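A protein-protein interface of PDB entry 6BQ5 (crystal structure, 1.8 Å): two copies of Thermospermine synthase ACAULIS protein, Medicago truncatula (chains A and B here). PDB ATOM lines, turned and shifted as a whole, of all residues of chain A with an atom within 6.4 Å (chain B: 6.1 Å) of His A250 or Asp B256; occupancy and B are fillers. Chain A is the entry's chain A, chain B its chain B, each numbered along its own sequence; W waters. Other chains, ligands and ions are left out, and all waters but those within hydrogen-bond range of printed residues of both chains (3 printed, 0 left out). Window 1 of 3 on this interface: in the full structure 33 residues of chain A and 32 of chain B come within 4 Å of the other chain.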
ATOM      1  N   ILE A  86     -19.143   7.222   8.379  1.00  0.00           N
ATOM      2  CA  ILE A  86     -20.265   8.114   8.437  1.00  0.00           C
ATOM      3  C   ILE A  86     -20.639   8.576   7.017  1.00  0.00           C
ATOM      4  O   ILE A  86     -21.789   8.412   6.601  1.00  0.00           O
ATOM      5  CB  ILE A  86     -20.006   9.317   9.349  1.00  0.00           C
ATOM      6  CG1 ILE A  86     -19.668   8.833  10.733  1.00  0.00           C
ATOM      7  CG2 ILE A  86     -21.200  10.287   9.340  1.00  0.00           C
ATOM      8  CD1 ILE A  86     -19.281   9.906  11.726  1.00  0.00           C
ATOM      9  N   SER A 248     -28.440  15.351   6.022  1.00  0.00           N
ATOM     10  CA  SER A 248     -27.096  15.747   6.419  1.00  0.00           C
ATOM     11  C   SER A 248     -26.611  15.096   7.703  1.00  0.00           C
ATOM     12  O   SER A 248     -27.399  14.591   8.459  1.00  0.00           O
ATOM     13  CB  SER A 248     -26.983  17.255   6.465  1.00  0.00           C
ATOM     14  OG  SER A 248     -27.747  17.797   7.523  1.00  0.00           O
ATOM     15  N   ALA A 249     -25.288  15.081   7.898  1.00  0.00           N
ATOM     16  CA  ALA A 249     -24.657  14.535   9.070  1.00  0.00           C
ATOM     17  C   ALA A 249     -23.277  15.184   9.270  1.00  0.00           C
ATOM     18  O   ALA A 249     -22.565  15.520   8.320  1.00  0.00           O
ATOM     19  CB  ALA A 249     -24.563  13.005   8.987  1.00  0.00           C
ATOM     20  N   HIS A 250     -22.899  15.333  10.542  1.00  0.00           N
ATOM     21  CA  HIS A 250     -21.574  15.830  10.920  1.00  0.00           C
ATOM     22  C   HIS A 250     -20.490  14.785  10.602  1.00  0.00           C
ATOM     23  O   HIS A 250     -20.621  13.578  10.960  1.00  0.00           O
ATOM     24  CB  HIS A 250     -21.538  16.091  12.412  1.00  0.00           C
ATOM     25  CG  HIS A 250     -20.242  16.633  12.908  1.00  0.00           C
ATOM     26  ND1 HIS A 250     -19.554  16.062  13.964  1.00  0.00           N
ATOM     27  CD2 HIS A 250     -19.522  17.723  12.529  1.00  0.00           C
ATOM     28  CE1 HIS A 250     -18.480  16.785  14.208  1.00  0.00           C
ATOM     29  NE2 HIS A 250     -18.416  17.772  13.333  1.00  0.00           N
ATOM     30  N   ILE A 251     -19.415  15.265   9.995  1.00  0.00           N
ATOM     31  CA  ILE A 251     -18.221  14.451   9.770  1.00  0.00           C
ATOM     32  C   ILE A 251     -17.048  15.089  10.524  1.00  0.00           C
ATOM     33  O   ILE A 251     -16.552  16.128  10.130  1.00  0.00           O
ATOM     34  CB  ILE A 251     -17.946  14.300   8.264  1.00  0.00           C
ATOM     35  CG1 ILE A 251     -19.158  13.639   7.603  1.00  0.00           C
ATOM     36  CG2 ILE A 251     -16.744  13.406   8.043  1.00  0.00           C
ATOM     37  CD1 ILE A 251     -19.093  13.684   6.122  1.00  0.00           C
ATOM     38  N   PRO A 252     -16.647  14.499  11.640  1.00  0.00           N
ATOM     39  CA  PRO A 252     -15.626  15.151  12.475  1.00  0.00           C
ATOM     40  C   PRO A 252     -14.380  15.634  11.701  1.00  0.00           C
ATOM     41  O   PRO A 252     -13.922  16.804  11.907  1.00  0.00           O
ATOM     42  CB  PRO A 252     -15.254  14.068  13.488  1.00  0.00           C
ATOM     43  CG  PRO A 252     -16.534  13.311  13.639  1.00  0.00           C
ATOM     44  CD  PRO A 252     -17.149  13.259  12.249  1.00  0.00           C
ATOM     45  N   SER A 253     -13.896  14.787  10.791  1.00  0.00           N
ATOM     46  CA  SER A 253     -12.636  15.077  10.110  1.00  0.00           C
ATOM     47  C   SER A 253     -12.746  16.239   9.131  1.00  0.00           C
ATOM     48  O   SER A 253     -11.714  16.854   8.765  1.00  0.00           O
ATOM     49  CB  SER A 253     -12.042  13.831   9.425  1.00  0.00           C
ATOM     50  OG  SER A 253     -12.897  13.341   8.432  1.00  0.00           O
ATOM     51  N   TYR A 254     -13.971  16.520   8.695  1.00  0.00           N
ATOM     52  CA  TYR A 254     -14.252  17.685   7.832  1.00  0.00           C
ATOM     53  C   TYR A 254     -14.547  18.955   8.603  1.00  0.00           C
ATOM     54  O   TYR A 254     -14.695  20.017   8.012  1.00  0.00           O
ATOM     55  CB  TYR A 254     -15.467  17.397   7.009  1.00  0.00           C
ATOM     56  CG  TYR A 254     -15.350  16.370   5.956  1.00  0.00           C
ATOM     57  CD1 TYR A 254     -14.209  15.585   5.809  1.00  0.00           C
ATOM     58  CD2 TYR A 254     -16.392  16.184   5.076  1.00  0.00           C
ATOM     59  CE1 TYR A 254     -14.151  14.636   4.807  1.00  0.00           C
ATOM     60  CE2 TYR A 254     -16.340  15.249   4.066  1.00  0.00           C
ATOM     61  CZ  TYR A 254     -15.230  14.465   3.939  1.00  0.00           C
ATOM     62  OH  TYR A 254     -15.164  13.476   2.979  1.00  0.00           O
ATOM     63  N   ALA A 255     -14.640  18.892   9.920  1.00  0.00           N
ATOM     64  CA  ALA A 255     -15.070  20.051  10.744  1.00  0.00           C
ATOM     65  C   ALA A 255     -16.304  20.772  10.152  1.00  0.00           C
ATOM     66  O   ALA A 255     -16.464  22.020  10.265  1.00  0.00           O
ATOM     67  CB  ALA A 255     -13.935  21.052  11.000  1.00  0.00           C
ATOM     68  N   ASP A 256     -17.233  19.984   9.604  1.00  0.00           N
ATOM     69  CA  ASP A 256     -18.493  20.568   9.075  1.00  0.00           C
ATOM     70  C   ASP A 256     -19.506  19.459   9.008  1.00  0.00           C
ATOM     71  O   ASP A 256     -19.184  18.233   9.127  1.00  0.00           O
ATOM     72  CB  ASP A 256     -18.265  21.192   7.675  1.00  0.00           C
ATOM     73  CG  ASP A 256     -19.275  22.293   7.309  1.00  0.00           C
ATOM     74  OD1 ASP A 256     -20.249  22.501   8.070  1.00  0.00           O
ATOM     75  OD2 ASP A 256     -19.075  22.945   6.270  1.00  0.00           O
ATOM     76  N   ILE A 257     -20.726  19.896   8.774  1.00  0.00           N
ATOM     77  CA  ILE A 257     -21.830  19.039   8.404  1.00  0.00           C
ATOM     78  C   ILE A 257     -21.706  18.814   6.909  1.00  0.00           C
ATOM     79  O   ILE A 257     -21.445  19.760   6.152  1.00  0.00           O
ATOM     80  CB  ILE A 257     -23.170  19.715   8.672  1.00  0.00           C
ATOM     81  CG1 ILE A 257     -23.298  20.189  10.141  1.00  0.00           C
ATOM     82  CG2 ILE A 257     -24.332  18.780   8.338  1.00  0.00           C
ATOM     83  CD1 ILE A 257     -22.998  19.153  11.182  1.00  0.00           C
ATOM     84  N   TRP A 258     -21.957  17.580   6.483  1.00  0.00           N
ATOM     85  CA  TRP A 258     -22.003  17.275   5.102  1.00  0.00           C
ATOM     86  C   TRP A 258     -23.414  16.876   4.656  1.00  0.00           C
ATOM     87  O   TRP A 258     -24.199  16.324   5.428  1.00  0.00           O
ATOM     88  CB  TRP A 258     -21.021  16.146   4.773  1.00  0.00           C
ATOM     89  CG  TRP A 258     -20.473  16.238   3.440  1.00  0.00           C
ATOM     90  CD1 TRP A 258     -20.816  15.520   2.366  1.00  0.00           C
ATOM     91  CD2 TRP A 258     -19.488  17.162   3.019  1.00  0.00           C
ATOM     92  NE1 TRP A 258     -20.086  15.899   1.294  1.00  0.00           N
ATOM     93  CE2 TRP A 258     -19.258  16.918   1.661  1.00  0.00           C
ATOM     94  CE3 TRP A 258     -18.779  18.171   3.660  1.00  0.00           C
ATOM     95  CZ2 TRP A 258     -18.388  17.678   0.905  1.00  0.00           C
ATOM     96  CZ3 TRP A 258     -17.858  18.900   2.920  1.00  0.00           C
ATOM     97  CH2 TRP A 258     -17.682  18.645   1.547  1.00  0.00           C
ATOM     98  N   TRP A 260     -26.236  15.156   1.554  1.00  0.00           N
ATOM     99  CA  TRP A 260     -26.565  14.220   0.447  1.00  0.00           C
ATOM    100  C   TRP A 260     -27.986  14.492   0.001  1.00  0.00           C
ATOM    101  O   TRP A 260     -28.772  15.084   0.754  1.00  0.00           O
ATOM    102  CB  TRP A 260     -26.435  12.726   0.915  1.00  0.00           C
ATOM    103  CG  TRP A 260     -25.077  12.422   1.476  1.00  0.00           C
ATOM    104  CD1 TRP A 260     -24.006  11.967   0.797  1.00  0.00           C
ATOM    105  CD2 TRP A 260     -24.654  12.579   2.831  1.00  0.00           C
ATOM    106  NE1 TRP A 260     -22.921  11.841   1.627  1.00  0.00           N
ATOM    107  CE2 TRP A 260     -23.295  12.205   2.890  1.00  0.00           C
ATOM    108  CE3 TRP A 260     -25.303  12.946   4.023  1.00  0.00           C
ATOM    109  CZ2 TRP A 260     -22.552  12.256   4.064  1.00  0.00           C
ATOM    110  CZ3 TRP A 260     -24.554  13.001   5.196  1.00  0.00           C
ATOM    111  CH2 TRP A 260     -23.203  12.660   5.214  1.00  0.00           C
ATOM    112  N   TYR A 289     -23.020   3.753  12.024  1.00  0.00           N
ATOM    113  CA  TYR A 289     -23.515   5.108  12.184  1.00  0.00           C
ATOM    114  C   TYR A 289     -25.032   5.161  12.138  1.00  0.00           C
ATOM    115  O   TYR A 289     -25.685   5.782  12.992  1.00  0.00           O
ATOM    116  CB  TYR A 289     -22.951   6.045  11.115  1.00  0.00           C
ATOM    117  CG  TYR A 289     -23.492   7.424  11.310  1.00  0.00           C
ATOM    118  CD1 TYR A 289     -23.095   8.223  12.379  1.00  0.00           C
ATOM    119  CD2 TYR A 289     -24.452   7.910  10.464  1.00  0.00           C
ATOM    120  CE1 TYR A 289     -23.645   9.506  12.552  1.00  0.00           C
ATOM    121  CE2 TYR A 289     -24.990   9.156  10.634  1.00  0.00           C
ATOM    122  CZ  TYR A 289     -24.626   9.931  11.679  1.00  0.00           C
ATOM    123  OH  TYR A 289     -25.271  11.175  11.724  1.00  0.00           O
ATOM    124  N   ILE B  35      -7.943  21.699  20.096  1.00  0.00           N
ATOM    125  CA  ILE B  35      -9.289  21.238  20.465  1.00  0.00           C
ATOM    126  C   ILE B  35      -9.305  19.918  21.234  1.00  0.00           C
ATOM    127  O   ILE B  35      -9.979  19.783  22.236  1.00  0.00           O
ATOM    128  CB  ILE B  35     -10.150  20.976  19.222  1.00  0.00           C
ATOM    129  CG1 ILE B  35     -10.540  22.270  18.586  1.00  0.00           C
ATOM    130  CG2 ILE B  35     -11.438  20.180  19.563  1.00  0.00           C
ATOM    131  CD1 ILE B  35     -10.852  22.004  17.144  1.00  0.00           C
ATOM    132  N   PRO B 220     -19.131  18.512  24.708  1.00  0.00           N
ATOM    133  CA  PRO B 220     -19.118  17.977  23.342  1.00  0.00           C
ATOM    134  C   PRO B 220     -20.089  16.811  23.145  1.00  0.00           C
ATOM    135  O   PRO B 220     -20.277  15.972  24.058  1.00  0.00           O
ATOM    136  CB  PRO B 220     -17.680  17.507  23.154  1.00  0.00           C
ATOM    137  CG  PRO B 220     -16.879  18.119  24.241  1.00  0.00           C
ATOM    138  CD  PRO B 220     -17.792  18.476  25.342  1.00  0.00           C
ATOM    139  N   ALA B 221     -20.690  16.731  21.967  1.00  0.00           N
ATOM    140  CA  ALA B 221     -21.659  15.682  21.698  1.00  0.00           C
ATOM    141  C   ALA B 221     -21.401  15.087  20.320  1.00  0.00           C
ATOM    142  O   ALA B 221     -22.310  14.594  19.652  1.00  0.00           O
ATOM    143  CB  ALA B 221     -23.098  16.218  21.848  1.00  0.00           C
ATOM    144  N   GLY B 222     -20.132  15.076  19.930  1.00  0.00           N
ATOM    145  CA  GLY B 222     -19.751  14.481  18.652  1.00  0.00           C
ATOM    146  C   GLY B 222     -19.780  12.960  18.724  1.00  0.00           C
ATOM    147  O   GLY B 222     -19.941  12.345  19.803  1.00  0.00           O
ATOM    148  N   ILE B 223     -19.648  12.358  17.559  1.00  0.00           N
ATOM    149  CA  ILE B 223     -19.718  10.905  17.433  1.00  0.00           C
ATOM    150  C   ILE B 223     -18.705  10.204  18.327  1.00  0.00           C
ATOM    151  O   ILE B 223     -19.059   9.185  18.960  1.00  0.00           O
ATOM    152  CB  ILE B 223     -19.663  10.493  15.946  1.00  0.00           C
ATOM    153  CG1 ILE B 223     -19.962   9.012  15.726  1.00  0.00           C
ATOM    154  CG2 ILE B 223     -18.348  10.851  15.322  1.00  0.00           C
ATOM    155  CD1 ILE B 223     -21.375   8.624  16.009  1.00  0.00           C
ATOM    156  N   SER B 225     -16.701  12.324  20.643  1.00  0.00           N
ATOM    157  CA  SER B 225     -16.485  13.189  21.796  1.00  0.00           C
ATOM    158  C   SER B 225     -17.621  13.127  22.848  1.00  0.00           C
ATOM    159  O   SER B 225     -17.428  13.574  24.015  1.00  0.00           O
ATOM    160  CB  SER B 225     -16.205  14.616  21.321  1.00  0.00           C
ATOM    161  OG  SER B 225     -17.343  15.215  20.666  1.00  0.00           O
ATOM    162  N   GLU B 228     -17.106  11.978  26.647  1.00  0.00           N
ATOM    163  CA  GLU B 228     -16.271  12.677  27.617  1.00  0.00           C
ATOM    164  C   GLU B 228     -17.058  13.136  28.833  1.00  0.00           C
ATOM    165  O   GLU B 228     -16.650  12.877  29.955  1.00  0.00           O
ATOM    166  CB  GLU B 228     -15.592  13.917  27.022  1.00  0.00           C
ATOM    167  CG  GLU B 228     -14.600  13.712  25.884  1.00  0.00           C
ATOM    168  CD  GLU B 228     -14.173  15.069  25.298  1.00  0.00           C
ATOM    169  OE1 GLU B 228     -13.963  16.044  26.106  1.00  0.00           O
ATOM    170  OE2 GLU B 228     -14.086  15.185  24.049  1.00  0.00           O
ATOM    171  N   ALA B 249     -26.385  20.056  18.765  1.00  0.00           N
ATOM    172  CA  ALA B 249     -26.337  20.829  17.546  1.00  0.00           C
ATOM    173  C   ALA B 249     -24.908  21.196  17.244  1.00  0.00           C
ATOM    174  O   ALA B 249     -24.068  21.405  18.145  1.00  0.00           O
ATOM    175  CB  ALA B 249     -27.152  22.107  17.685  1.00  0.00           C
ATOM    176  N   HIS B 250     -24.625  21.312  15.976  1.00  0.00           N
ATOM    177  CA  HIS B 250     -23.310  21.731  15.536  1.00  0.00           C
ATOM    178  C   HIS B 250     -23.081  23.236  15.800  1.00  0.00           C
ATOM    179  O   HIS B 250     -23.933  24.058  15.501  1.00  0.00           O
ATOM    180  CB  HIS B 250     -23.182  21.424  14.047  1.00  0.00           C
ATOM    181  CG  HIS B 250     -21.856  21.790  13.439  1.00  0.00           C
ATOM    182  ND1 HIS B 250     -21.756  22.574  12.316  1.00  0.00           N
ATOM    183  CD2 HIS B 250     -20.591  21.416  13.757  1.00  0.00           C
ATOM    184  CE1 HIS B 250     -20.478  22.745  12.012  1.00  0.00           C
ATOM    185  NE2 HIS B 250     -19.740  22.061  12.876  1.00  0.00           N
ATOM    186  N   ILE B 251     -21.890  23.564  16.299  1.00  0.00           N
ATOM    187  CA  ILE B 251     -21.443  24.952  16.391  1.00  0.00           C
ATOM    188  C   ILE B 251     -20.151  25.081  15.579  1.00  0.00           C
ATOM    189  O   ILE B 251     -19.134  24.567  15.968  1.00  0.00           O
ATOM    190  CB  ILE B 251     -21.264  25.337  17.848  1.00  0.00           C
ATOM    191  CG1 ILE B 251     -22.545  24.877  18.569  1.00  0.00           C
ATOM    192  CG2 ILE B 251     -20.933  26.823  17.942  1.00  0.00           C
ATOM    193  CD1 ILE B 251     -22.815  25.526  19.847  1.00  0.00           C
ATOM    194  N   PRO B 252     -20.200  25.768  14.448  1.00  0.00           N
ATOM    195  CA  PRO B 252     -19.002  25.757  13.557  1.00  0.00           C
ATOM    196  C   PRO B 252     -17.714  26.203  14.229  1.00  0.00           C
ATOM    197  O   PRO B 252     -16.674  25.546  14.104  1.00  0.00           O
ATOM    198  CB  PRO B 252     -19.364  26.724  12.451  1.00  0.00           C
ATOM    199  CG  PRO B 252     -20.877  26.592  12.365  1.00  0.00           C
ATOM    200  CD  PRO B 252     -21.384  26.370  13.778  1.00  0.00           C
ATOM    201  N   SER B 253     -17.779  27.257  15.014  1.00  0.00           N
ATOM    202  CA  SER B 253     -16.571  27.760  15.651  1.00  0.00           C
ATOM    203  C   SER B 253     -15.963  26.772  16.692  1.00  0.00           C
ATOM    204  O   SER B 253     -14.785  26.907  17.041  1.00  0.00           O
ATOM    205  CB  SER B 253     -16.859  29.124  16.287  1.00  0.00           C
ATOM    206  OG  SER B 253     -17.750  29.016  17.343  1.00  0.00           O
ATOM    207  N   TYR B 254     -16.755  25.830  17.193  1.00  0.00           N
ATOM    208  CA  TYR B 254     -16.318  24.855  18.194  1.00  0.00           C
ATOM    209  C   TYR B 254     -15.714  23.662  17.548  1.00  0.00           C
ATOM    210  O   TYR B 254     -15.168  22.847  18.263  1.00  0.00           O
ATOM    211  CB  TYR B 254     -17.486  24.348  19.062  1.00  0.00           C
ATOM    212  CG  TYR B 254     -18.040  25.284  20.072  1.00  0.00           C
ATOM    213  CD1 TYR B 254     -17.741  26.670  20.068  1.00  0.00           C
ATOM    214  CD2 TYR B 254     -18.813  24.806  21.080  1.00  0.00           C
ATOM    215  CE1 TYR B 254     -18.295  27.529  21.026  1.00  0.00           C
ATOM    216  CE2 TYR B 254     -19.346  25.630  22.068  1.00  0.00           C
ATOM    217  CZ  TYR B 254     -19.116  26.979  22.039  1.00  0.00           C
ATOM    218  OH  TYR B 254     -19.693  27.748  23.027  1.00  0.00           O
ATOM    219  N   ALA B 255     -15.848  23.510  16.229  1.00  0.00           N
ATOM    220  CA  ALA B 255     -15.336  22.352  15.517  1.00  0.00           C
ATOM    221  C   ALA B 255     -15.914  21.025  16.079  1.00  0.00           C
ATOM    222  O   ALA B 255     -15.238  19.985  16.118  1.00  0.00           O
ATOM    223  CB  ALA B 255     -13.822  22.356  15.572  1.00  0.00           C
ATOM    224  N   ASP B 256     -17.161  21.079  16.505  1.00  0.00           N
ATOM    225  CA  ASP B 256     -17.846  19.901  17.068  1.00  0.00           C
ATOM    226  C   ASP B 256     -19.307  20.183  17.212  1.00  0.00           C
ATOM    227  O   ASP B 256     -19.774  21.332  17.082  1.00  0.00           O
ATOM    228  CB  ASP B 256     -17.280  19.552  18.471  1.00  0.00           C
ATOM    229  CG  ASP B 256     -17.273  18.044  18.777  1.00  0.00           C
ATOM    230  OD1 ASP B 256     -17.965  17.253  18.038  1.00  0.00           O
ATOM    231  OD2 ASP B 256     -16.601  17.682  19.759  1.00  0.00           O
ATOM    232  N   ILE B 257     -20.007  19.111  17.469  1.00  0.00           N
ATOM    233  CA  ILE B 257     -21.370  19.105  17.958  1.00  0.00           C
ATOM    234  C   ILE B 257     -21.308  19.413  19.455  1.00  0.00           C
ATOM    235  O   ILE B 257     -20.484  18.851  20.196  1.00  0.00           O
ATOM    236  CB  ILE B 257     -22.031  17.720  17.796  1.00  0.00           C
ATOM    237  CG1 ILE B 257     -21.967  17.202  16.365  1.00  0.00           C
ATOM    238  CG2 ILE B 257     -23.476  17.745  18.190  1.00  0.00           C
ATOM    239  CD1 ILE B 257     -22.434  18.161  15.317  1.00  0.00           C
ATOM    240  N   TRP B 258     -22.194  20.288  19.894  1.00  0.00           N
ATOM    241  CA  TRP B 258     -22.331  20.538  21.325  1.00  0.00           C
ATOM    242  C   TRP B 258     -23.641  19.963  21.850  1.00  0.00           C
ATOM    243  O   TRP B 258     -24.624  19.834  21.107  1.00  0.00           O
ATOM    244  CB  TRP B 258     -22.197  22.043  21.624  1.00  0.00           C
ATOM    245  CG  TRP B 258     -21.556  22.290  22.896  1.00  0.00           C
ATOM    246  CD1 TRP B 258     -22.144  22.703  24.031  1.00  0.00           C
ATOM    247  CD2 TRP B 258     -20.189  22.150  23.169  1.00  0.00           C
ATOM    248  NE1 TRP B 258     -21.217  22.800  25.035  1.00  0.00           N
ATOM    249  CE2 TRP B 258     -20.006  22.438  24.525  1.00  0.00           C
ATOM    250  CE3 TRP B 258     -19.108  21.706  22.418  1.00  0.00           C
ATOM    251  CZ2 TRP B 258     -18.761  22.336  25.163  1.00  0.00           C
ATOM    252  CZ3 TRP B 258     -17.844  21.641  23.032  1.00  0.00           C
ATOM    253  CH2 TRP B 258     -17.694  21.970  24.393  1.00  0.00           C
HETATM  254  O   HOH W   1     -16.926  23.109  12.663  1.00  0.00           O
HETATM  255  O   HOH W   2     -20.506  13.896  15.317  1.00  0.00           O
HETATM  256  O   HOH W   3     -15.463  18.479  13.533  1.00  0.00           O
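O of Ile B257 is in hydrogen-bond range of N of Ala B221 (2.8 Å). N of Ile B251 sits at hydrogen-bond distance from O of Asp B256 (3.2 Å). The side-chain carboxylate (OD2) of Asp B256 lies within hydrogen-bond range of the side-chain hydroxyl (OG) of Ser B225, 2.7 Å away. The backbone carbonyl oxygen (O) of Asp A256 is in hydrogen-bond range of the backbone NH (N) of Ile A251, at 3.1 Å.
Ile A86 touches Ile B223. Asp B256 touches His A250 (OD1 to CE1, 3.9 Å). ND1 of His A250 touches CG1 of Ile B257 (3.6 Å). Pro A252 touches Ile B223 (CG to CG2, 3.5 Å). Asp A256 touches His B250. CG1 of Ile A257 touches ND1 of His B250 (3.6 Å).
Of chain B, only Asp B256 and Ile B257 come within 4 Å of His A250. Asp B256 touches one residue of chain A. Of the printed residues of chain A, Ile B223 touches Ile A86 and Pro A252. Of the printed residues of chain A, Ile B257 touches His A250 (3.6 Å). Tyr B254 touches none of the printed residues of chain A. Tyr A289 touches none of the printed residues of chain B. The nearest residue of chain B that does not touch His A250 is His B250 (4.04 Å). The nearest residue of chain A that does not touch Asp B256 is Pro A252 (6.1 Å). The nearest printed residue of chain B that does not touch Ile A257 is Ile B257 (4.3 Å).
Of the 17 printed residues of chain B, 4 touch a printed residue of chain A. Printed residues of chain B that touch a printed residue of chain A: Ile B223, His B250, Asp B256 and Ile B257. Along chain B the printed residues that touch a printed residue of chain A span positions 223 to 257. Among the printed residues, no Asp or Glu carboxylate lies within 4 Å of a Lys or Arg side-chain nitrogen of the other chain.
His A250 touches Asp B256, and with the chains exchanged Asp A256 touches His B250. His A250 touches Ile B257, and with the chains exchanged Ile A257 touches His B250. Of the 6 pairs that touch across the chains among the printed residues, 4 have their exchanged pair printed and touching as well.
Water W1 lies within hydrogen-bond range of the backbone carbonyl oxygen of Ala A255 (2.7 Å), the backbone carbonyl oxygen of Pro B252 (2.8 Å) and a ring nitrogen (NE2) of His B250 (3.0 Å). Water W2 bridges ND1 of His A250 and N of Ile B223. Water W3 lies within hydrogen-bond range of the backbone carbonyl oxygen (O) of Pro A252, the backbone carbonyl oxygen (O) of Ala B255 and a ring nitrogen (NE2) of His A250.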
